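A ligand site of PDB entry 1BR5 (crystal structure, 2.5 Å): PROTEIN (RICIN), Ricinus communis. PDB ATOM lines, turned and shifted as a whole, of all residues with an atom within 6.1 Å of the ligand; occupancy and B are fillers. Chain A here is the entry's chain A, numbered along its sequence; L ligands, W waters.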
ATOM      1  N   LEU A  74     -17.337  17.129 -29.047  1.00  0.00           N
ATOM      2  CA  LEU A  74     -18.504  17.043 -28.158  1.00  0.00           C
ATOM      3  C   LEU A  74     -18.930  15.594 -28.010  1.00  0.00           C
ATOM      4  O   LEU A  74     -19.088  14.868 -28.987  1.00  0.00           O
ATOM      5  CB  LEU A  74     -19.751  17.802 -28.713  1.00  0.00           C
ATOM      6  CG  LEU A  74     -20.055  19.304 -28.598  1.00  0.00           C
ATOM      7  CD1 LEU A  74     -20.427  19.626 -27.187  1.00  0.00           C
ATOM      8  CD2 LEU A  74     -18.861  20.143 -28.998  1.00  0.00           C
ATOM      9  N   ASN A  78     -23.577  13.528 -23.251  1.00  0.00           N
ATOM     10  CA  ASN A  78     -23.674  14.558 -22.206  1.00  0.00           C
ATOM     11  C   ASN A  78     -23.331  15.979 -22.666  1.00  0.00           C
ATOM     12  O   ASN A  78     -23.298  16.931 -21.878  1.00  0.00           O
ATOM     13  CB  ASN A  78     -22.757  14.186 -20.986  1.00  0.00           C
ATOM     14  CG  ASN A  78     -21.264  13.989 -21.236  1.00  0.00           C
ATOM     15  OD1 ASN A  78     -20.719  14.159 -22.316  1.00  0.00           O
ATOM     16  ND2 ASN A  78     -20.507  13.603 -20.231  1.00  0.00           N
ATOM     17  N   ALA A  79     -23.130  16.138 -23.971  1.00  0.00           N
ATOM     18  CA  ALA A  79     -22.639  17.341 -24.599  1.00  0.00           C
ATOM     19  C   ALA A  79     -21.353  17.873 -23.982  1.00  0.00           C
ATOM     20  O   ALA A  79     -21.022  19.021 -24.202  1.00  0.00           O
ATOM     21  CB  ALA A  79     -23.703  18.452 -24.551  1.00  0.00           C
ATOM     22  N   TYR A  80     -20.557  17.069 -23.286  1.00  0.00           N
ATOM     23  CA  TYR A  80     -19.269  17.490 -22.751  1.00  0.00           C
ATOM     24  C   TYR A  80     -18.223  17.829 -23.808  1.00  0.00           C
ATOM     25  O   TYR A  80     -18.057  17.081 -24.761  1.00  0.00           O
ATOM     26  CB  TYR A  80     -18.695  16.389 -21.887  1.00  0.00           C
ATOM     27  CG  TYR A  80     -17.743  16.747 -20.748  1.00  0.00           C
ATOM     28  CD1 TYR A  80     -18.247  17.002 -19.462  1.00  0.00           C
ATOM     29  CD2 TYR A  80     -16.349  16.766 -20.973  1.00  0.00           C
ATOM     30  CE1 TYR A  80     -17.370  17.246 -18.394  1.00  0.00           C
ATOM     31  CE2 TYR A  80     -15.470  17.017 -19.912  1.00  0.00           C
ATOM     32  CZ  TYR A  80     -15.980  17.260 -18.644  1.00  0.00           C
ATOM     33  OH  TYR A  80     -15.078  17.469 -17.633  1.00  0.00           O
ATOM     34  N   VAL A  81     -17.459  18.903 -23.672  1.00  0.00           N
ATOM     35  CA  VAL A  81     -16.361  19.246 -24.575  1.00  0.00           C
ATOM     36  C   VAL A  81     -15.188  18.342 -24.132  1.00  0.00           C
ATOM     37  O   VAL A  81     -14.614  18.540 -23.055  1.00  0.00           O
ATOM     38  CB  VAL A  81     -15.988  20.751 -24.442  1.00  0.00           C
ATOM     39  CG1 VAL A  81     -14.752  21.104 -25.278  1.00  0.00           C
ATOM     40  CG2 VAL A  81     -17.187  21.585 -24.902  1.00  0.00           C
ATOM     41  N   VAL A  82     -14.823  17.313 -24.899  1.00  0.00           N
ATOM     42  CA  VAL A  82     -13.772  16.400 -24.467  1.00  0.00           C
ATOM     43  C   VAL A  82     -12.383  16.841 -24.942  1.00  0.00           C
ATOM     44  O   VAL A  82     -11.390  16.390 -24.399  1.00  0.00           O
ATOM     45  CB  VAL A  82     -14.082  14.883 -24.954  1.00  0.00           C
ATOM     46  CG1 VAL A  82     -15.551  14.571 -24.683  1.00  0.00           C
ATOM     47  CG2 VAL A  82     -13.808  14.636 -26.425  1.00  0.00           C
ATOM     48  N   PHE A  93      -8.807  16.684 -22.703  1.00  0.00           N
ATOM     49  CA  PHE A  93      -8.652  16.739 -21.254  1.00  0.00           C
ATOM     50  C   PHE A  93      -8.244  15.334 -20.740  1.00  0.00           C
ATOM     51  O   PHE A  93      -8.284  14.378 -21.501  1.00  0.00           O
ATOM     52  CB  PHE A  93      -9.975  17.186 -20.624  1.00  0.00           C
ATOM     53  CG  PHE A  93     -10.331  18.643 -20.905  1.00  0.00           C
ATOM     54  CD1 PHE A  93      -9.610  19.679 -20.291  1.00  0.00           C
ATOM     55  CD2 PHE A  93     -11.408  18.958 -21.753  1.00  0.00           C
ATOM     56  CE1 PHE A  93      -9.953  21.006 -20.504  1.00  0.00           C
ATOM     57  CE2 PHE A  93     -11.738  20.301 -21.975  1.00  0.00           C
ATOM     58  CZ  PHE A  93     -11.009  21.315 -21.355  1.00  0.00           C
ATOM     59  N   GLY A 121     -11.409  18.281 -17.573  1.00  0.00           N
ATOM     60  CA  GLY A 121     -12.039  19.492 -18.069  1.00  0.00           C
ATOM     61  C   GLY A 121     -13.202  20.048 -17.301  1.00  0.00           C
ATOM     62  O   GLY A 121     -13.899  20.898 -17.825  1.00  0.00           O
ATOM     63  N   ASN A 122     -13.499  19.587 -16.106  1.00  0.00           N
ATOM     64  CA  ASN A 122     -14.626  20.132 -15.359  1.00  0.00           C
ATOM     65  C   ASN A 122     -14.229  21.468 -14.770  1.00  0.00           C
ATOM     66  O   ASN A 122     -13.088  21.720 -14.347  1.00  0.00           O
ATOM     67  CB  ASN A 122     -15.113  19.219 -14.192  1.00  0.00           C
ATOM     68  CG  ASN A 122     -14.145  18.132 -13.760  1.00  0.00           C
ATOM     69  OD1 ASN A 122     -13.167  18.376 -13.072  1.00  0.00           O
ATOM     70  ND2 ASN A 122     -14.296  16.894 -14.220  1.00  0.00           N
ATOM     71  N   TYR A 123     -15.224  22.342 -14.868  1.00  0.00           N
ATOM     72  CA  TYR A 123     -15.203  23.699 -14.303  1.00  0.00           C
ATOM     73  C   TYR A 123     -14.377  23.868 -13.044  1.00  0.00           C
ATOM     74  O   TYR A 123     -13.631  24.837 -13.037  1.00  0.00           O
ATOM     75  CB  TYR A 123     -16.618  24.206 -13.955  1.00  0.00           C
ATOM     76  CG  TYR A 123     -17.556  24.474 -15.134  1.00  0.00           C
ATOM     77  CD1 TYR A 123     -17.081  25.087 -16.300  1.00  0.00           C
ATOM     78  CD2 TYR A 123     -18.905  24.119 -15.007  1.00  0.00           C
ATOM     79  CE1 TYR A 123     -17.938  25.327 -17.358  1.00  0.00           C
ATOM     80  CE2 TYR A 123     -19.772  24.374 -16.066  1.00  0.00           C
ATOM     81  CZ  TYR A 123     -19.285  24.981 -17.236  1.00  0.00           C
ATOM     82  OH  TYR A 123     -20.149  25.253 -18.270  1.00  0.00           O
ATOM     83  N   LEU A 126     -10.778  23.701 -14.141  1.00  0.00           N
ATOM     84  CA  LEU A 126     -10.643  24.819 -15.028  1.00  0.00           C
ATOM     85  C   LEU A 126     -10.739  26.189 -14.373  1.00  0.00           C
ATOM     86  O   LEU A 126     -10.036  27.102 -14.791  1.00  0.00           O
ATOM     87  CB  LEU A 126     -11.689  24.602 -16.122  1.00  0.00           C
ATOM     88  CG  LEU A 126     -11.295  24.229 -17.578  1.00  0.00           C
ATOM     89  CD1 LEU A 126     -10.094  23.301 -17.632  1.00  0.00           C
ATOM     90  CD2 LEU A 126     -12.522  23.624 -18.225  1.00  0.00           C
ATOM     91  N   ARG A 134     -16.175  31.250 -12.646  1.00  0.00           N
ATOM     92  CA  ARG A 134     -17.210  31.472 -13.658  1.00  0.00           C
ATOM     93  C   ARG A 134     -17.980  32.776 -13.544  1.00  0.00           C
ATOM     94  O   ARG A 134     -18.218  33.434 -14.553  1.00  0.00           O
ATOM     95  CB  ARG A 134     -18.209  30.338 -13.650  1.00  0.00           C
ATOM     96  CG  ARG A 134     -17.801  29.166 -14.462  1.00  0.00           C
ATOM     97  CD  ARG A 134     -18.855  28.094 -14.283  1.00  0.00           C
ATOM     98  NE  ARG A 134     -18.657  27.291 -13.089  1.00  0.00           N
ATOM     99  CZ  ARG A 134     -19.645  26.625 -12.487  1.00  0.00           C
ATOM    100  NH1 ARG A 134     -20.897  26.656 -12.918  1.00  0.00           N
ATOM    101  NH2 ARG A 134     -19.347  25.832 -11.472  1.00  0.00           N
ATOM    102  N   PHE A 168     -11.623  27.730 -22.435  1.00  0.00           N
ATOM    103  CA  PHE A 168     -12.481  26.560 -22.454  1.00  0.00           C
ATOM    104  C   PHE A 168     -13.760  26.811 -21.720  1.00  0.00           C
ATOM    105  O   PHE A 168     -14.795  26.503 -22.307  1.00  0.00           O
ATOM    106  CB  PHE A 168     -11.858  25.345 -21.813  1.00  0.00           C
ATOM    107  CG  PHE A 168     -10.947  24.576 -22.764  1.00  0.00           C
ATOM    108  CD1 PHE A 168     -11.499  23.943 -23.892  1.00  0.00           C
ATOM    109  CD2 PHE A 168      -9.577  24.492 -22.508  1.00  0.00           C
ATOM    110  CE1 PHE A 168     -10.667  23.216 -24.739  1.00  0.00           C
ATOM    111  CE2 PHE A 168      -8.759  23.761 -23.382  1.00  0.00           C
ATOM    112  CZ  PHE A 168      -9.295  23.126 -24.491  1.00  0.00           C
ATOM    113  N   ILE A 172     -17.378  26.360 -23.260  1.00  0.00           N
ATOM    114  CA  ILE A 172     -18.300  25.352 -22.759  1.00  0.00           C
ATOM    115  C   ILE A 172     -19.698  25.958 -22.511  1.00  0.00           C
ATOM    116  O   ILE A 172     -20.714  25.358 -22.859  1.00  0.00           O
ATOM    117  CB  ILE A 172     -17.705  24.739 -21.457  1.00  0.00           C
ATOM    118  CG1 ILE A 172     -16.382  23.985 -21.736  1.00  0.00           C
ATOM    119  CG2 ILE A 172     -18.731  23.789 -20.872  1.00  0.00           C
ATOM    120  CD1 ILE A 172     -15.399  23.858 -20.526  1.00  0.00           C
ATOM    121  N   SER A 176     -22.051  24.137 -25.016  1.00  0.00           N
ATOM    122  CA  SER A 176     -22.747  23.008 -24.397  1.00  0.00           C
ATOM    123  C   SER A 176     -23.845  23.403 -23.405  1.00  0.00           C
ATOM    124  O   SER A 176     -24.869  22.723 -23.337  1.00  0.00           O
ATOM    125  CB  SER A 176     -21.694  22.116 -23.733  1.00  0.00           C
ATOM    126  OG  SER A 176     -20.611  21.739 -24.586  1.00  0.00           O
ATOM    127  N   GLU A 177     -23.741  24.503 -22.651  1.00  0.00           N
ATOM    128  CA  GLU A 177     -24.793  24.955 -21.757  1.00  0.00           C
ATOM    129  C   GLU A 177     -25.969  25.568 -22.505  1.00  0.00           C
ATOM    130  O   GLU A 177     -27.116  25.336 -22.161  1.00  0.00           O
ATOM    131  CB  GLU A 177     -24.202  25.958 -20.733  1.00  0.00           C
ATOM    132  CG  GLU A 177     -23.089  25.415 -19.823  1.00  0.00           C
ATOM    133  CD  GLU A 177     -23.349  24.170 -18.971  1.00  0.00           C
ATOM    134  OE1 GLU A 177     -24.434  23.603 -18.904  1.00  0.00           O
ATOM    135  OE2 GLU A 177     -22.431  23.751 -18.303  1.00  0.00           O
ATOM    136  N   ARG A 180     -27.898  22.543 -23.580  1.00  0.00           N
ATOM    137  CA  ARG A 180     -28.539  21.923 -22.452  1.00  0.00           C
ATOM    138  C   ARG A 180     -29.741  22.717 -22.003  1.00  0.00           C
ATOM    139  O   ARG A 180     -30.733  22.136 -21.626  1.00  0.00           O
ATOM    140  CB  ARG A 180     -27.636  21.817 -21.253  1.00  0.00           C
ATOM    141  CG  ARG A 180     -26.539  20.839 -21.503  1.00  0.00           C
ATOM    142  CD  ARG A 180     -25.555  20.828 -20.374  1.00  0.00           C
ATOM    143  NE  ARG A 180     -24.507  19.845 -20.594  1.00  0.00           N
ATOM    144  CZ  ARG A 180     -23.204  20.168 -20.590  1.00  0.00           C
ATOM    145  NH1 ARG A 180     -22.766  21.418 -20.392  1.00  0.00           N
ATOM    146  NH2 ARG A 180     -22.319  19.190 -20.778  1.00  0.00           N
ATOM    147  N   GLU A 208     -26.275  25.264 -14.582  1.00  0.00           N
ATOM    148  CA  GLU A 208     -25.077  24.527 -14.973  1.00  0.00           C
ATOM    149  C   GLU A 208     -24.751  23.456 -13.950  1.00  0.00           C
ATOM    150  O   GLU A 208     -24.427  22.324 -14.292  1.00  0.00           O
ATOM    151  CB  GLU A 208     -23.865  25.441 -15.049  1.00  0.00           C
ATOM    152  CG  GLU A 208     -23.870  26.355 -16.229  1.00  0.00           C
ATOM    153  CD  GLU A 208     -22.928  27.531 -16.180  1.00  0.00           C
ATOM    154  OE1 GLU A 208     -22.024  27.587 -15.373  1.00  0.00           O
ATOM    155  OE2 GLU A 208     -23.135  28.409 -16.990  1.00  0.00           O
ATOM    156  N   ASN A 209     -24.804  23.855 -12.688  1.00  0.00           N
ATOM    157  CA  ASN A 209     -24.469  22.957 -11.618  1.00  0.00           C
ATOM    158  C   ASN A 209     -25.457  21.879 -11.261  1.00  0.00           C
ATOM    159  O   ASN A 209     -25.051  20.869 -10.658  1.00  0.00           O
ATOM    160  CB  ASN A 209     -24.220  23.722 -10.361  1.00  0.00           C
ATOM    161  CG  ASN A 209     -23.050  24.649 -10.432  1.00  0.00           C
ATOM    162  OD1 ASN A 209     -22.941  25.564  -9.620  1.00  0.00           O
ATOM    163  ND2 ASN A 209     -22.121  24.484 -11.365  1.00  0.00           N
ATOM    164  N   SER A 210     -26.722  22.134 -11.599  1.00  0.00           N
ATOM    165  CA  SER A 210     -27.847  21.252 -11.304  1.00  0.00           C
ATOM    166  C   SER A 210     -28.377  20.379 -12.443  1.00  0.00           C
ATOM    167  O   SER A 210     -29.333  19.651 -12.201  1.00  0.00           O
ATOM    168  CB  SER A 210     -28.960  22.137 -10.761  1.00  0.00           C
ATOM    169  OG  SER A 210     -28.497  22.937  -9.686  1.00  0.00           O
ATOM    170  N   TRP A 211     -27.829  20.372 -13.656  1.00  0.00           N
ATOM    171  CA  TRP A 211     -28.319  19.613 -14.784  1.00  0.00           C
ATOM    172  C   TRP A 211     -28.419  18.102 -14.580  1.00  0.00           C
ATOM    173  O   TRP A 211     -29.379  17.481 -15.026  1.00  0.00           O
ATOM    174  CB  TRP A 211     -27.422  19.931 -15.943  1.00  0.00           C
ATOM    175  CG  TRP A 211     -27.803  19.315 -17.289  1.00  0.00           C
ATOM    176  CD1 TRP A 211     -28.982  19.642 -17.912  1.00  0.00           C
ATOM    177  CD2 TRP A 211     -26.981  18.313 -18.101  1.00  0.00           C
ATOM    178  NE1 TRP A 211     -29.048  18.988 -19.040  1.00  0.00           N
ATOM    179  CE2 TRP A 211     -27.983  18.200 -19.281  1.00  0.00           C
ATOM    180  CE3 TRP A 211     -25.792  17.569 -18.149  1.00  0.00           C
ATOM    181  CZ2 TRP A 211     -27.683  17.364 -20.350  1.00  0.00           C
ATOM    182  CZ3 TRP A 211     -25.562  16.751 -19.264  1.00  0.00           C
ATOM    183  CH2 TRP A 211     -26.482  16.661 -20.323  1.00  0.00           C
ATOM    184  N   GLY A 212     -27.465  17.476 -13.893  1.00  0.00           N
ATOM    185  CA  GLY A 212     -27.502  16.055 -13.653  1.00  0.00           C
ATOM    186  C   GLY A 212     -28.693  15.673 -12.794  1.00  0.00           C
ATOM    187  O   GLY A 212     -29.514  14.810 -13.102  1.00  0.00           O
HETATM  188  N1  LIG L   1     -17.185  20.457 -21.052  1.00  0.00           N
HETATM  189  C1  LIG L   1     -18.426  20.524 -20.502  1.00  0.00           C
HETATM  190  C2  LIG L   1     -18.585  20.720 -19.118  1.00  0.00           C
HETATM  191  N2  LIG L   1     -19.774  20.825 -18.453  1.00  0.00           N
HETATM  192  C3  LIG L   1     -19.815  20.962 -17.082  1.00  0.00           C
HETATM  193  C4  LIG L   1     -18.573  21.012 -16.378  1.00  0.00           C
HETATM  194  N3  LIG L   1     -17.393  20.943 -17.048  1.00  0.00           N
HETATM  195  C5  LIG L   1     -17.372  20.801 -18.381  1.00  0.00           C
HETATM  196  N4  LIG L   1     -16.185  20.721 -18.962  1.00  0.00           N
HETATM  197  C6  LIG L   1     -16.065  20.558 -20.278  1.00  0.00           C
HETATM  198  N5  LIG L   1     -14.874  20.177 -20.720  1.00  0.00           N
HETATM  199  C7  LIG L   1     -21.198  21.065 -16.388  1.00  0.00           C
HETATM  200  O1  LIG L   1     -22.248  21.180 -17.344  1.00  0.00           O
HETATM  201  C8  LIG L   1     -21.605  19.956 -15.409  1.00  0.00           C
HETATM  202  O2  LIG L   1     -22.836  19.319 -15.848  1.00  0.00           O
HETATM  203  C9  LIG L   1     -21.789  20.446 -13.927  1.00  0.00           C
HETATM  204  O3  LIG L   1     -20.828  21.457 -13.518  1.00  0.00           O
HETATM  205  O4  LIG L   1     -19.505  20.208 -21.316  1.00  0.00           O
HETATM  206  O   HOH W   1     -18.301  20.471 -12.720  1.00  0.00           O
HETATM  207  O   HOH W   2     -25.112  21.244 -17.386  1.00  0.00           O
HETATM  208  O   HOH W   3     -24.832  18.428 -13.824  1.00  0.00           O
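N5 of the ligand sits at hydrogen-bond distance from O of Gly 121 (3.1 Å). OE2 of Glu 177 lies within hydrogen-bond range of O1 of the ligand (2.8 Å). N of Val 81 lies within hydrogen-bond range of O4 of the ligand (3.4 Å). A nitrogen (N5) of the ligand lies within hydrogen-bond range of the backbone carbonyl oxygen of Val 81, 2.9 Å away. The guanidinium group (NH2) of Arg 180 is in hydrogen-bond range of an oxygen (O4) of the ligand (3.0 Å). N of Tyr 123 sits at hydrogen-bond distance from N3 of the ligand (3.4 Å).
The backbone NH (N) of Glu 177 lies within hydrogen-bond range of the backbone carbonyl oxygen (O) of Ile 172 (3.2 Å). OH of Tyr 123 lies within hydrogen-bond range of OE2 of Glu 177, 2.7 Å away. O of Asn 78 sits at hydrogen-bond distance from NH2 of Arg 180 (2.7 Å). OH of Tyr 80 is in hydrogen-bond range of N of Asn 122 (3.1 Å). The backbone NH of Tyr 80 sits close to the side-chain amide oxygen of Asn 78, 3.1 Å away. The backbone NH (N) of Phe 93 sits at hydrogen-bond distance from the backbone carbonyl oxygen (O) of Val 82. The backbone carbonyl oxygen of Ala 79 sits at hydrogen-bond distance from the side-chain hydroxyl of Ser 176 (2.8 Å). The side-chain amide nitrogen of Asn 209 lies close to the guanidinium group of Arg 134 (2.9 Å).
An oxygen (O4) of the ligand lies close to the backbone carbonyl oxygen of Ala 79, 3.5 Å away. Residues that only touch the ligand: Tyr 80 (3.1 Å), Glu 208 (3.3 Å), Ile 172 (3.3 Å), Asn 122 (3.3 Å), Phe 93 (3.4 Å), Ser 176 (3.8 Å) and Asn 209 (3.9 Å). Hydrophobic or aromatic side chains within 4 Å of the ligand: Tyr 80, Val 81, Phe 93, Tyr 123 and Ile 172.
Water W2 lies within hydrogen-bond range of O1 of the ligand, OE1 of Glu 177 and O of Glu 208. Water W3 lies within hydrogen-bond range of N of Gly 212 (2.8 Å) and O2 of the ligand (3.0 Å).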
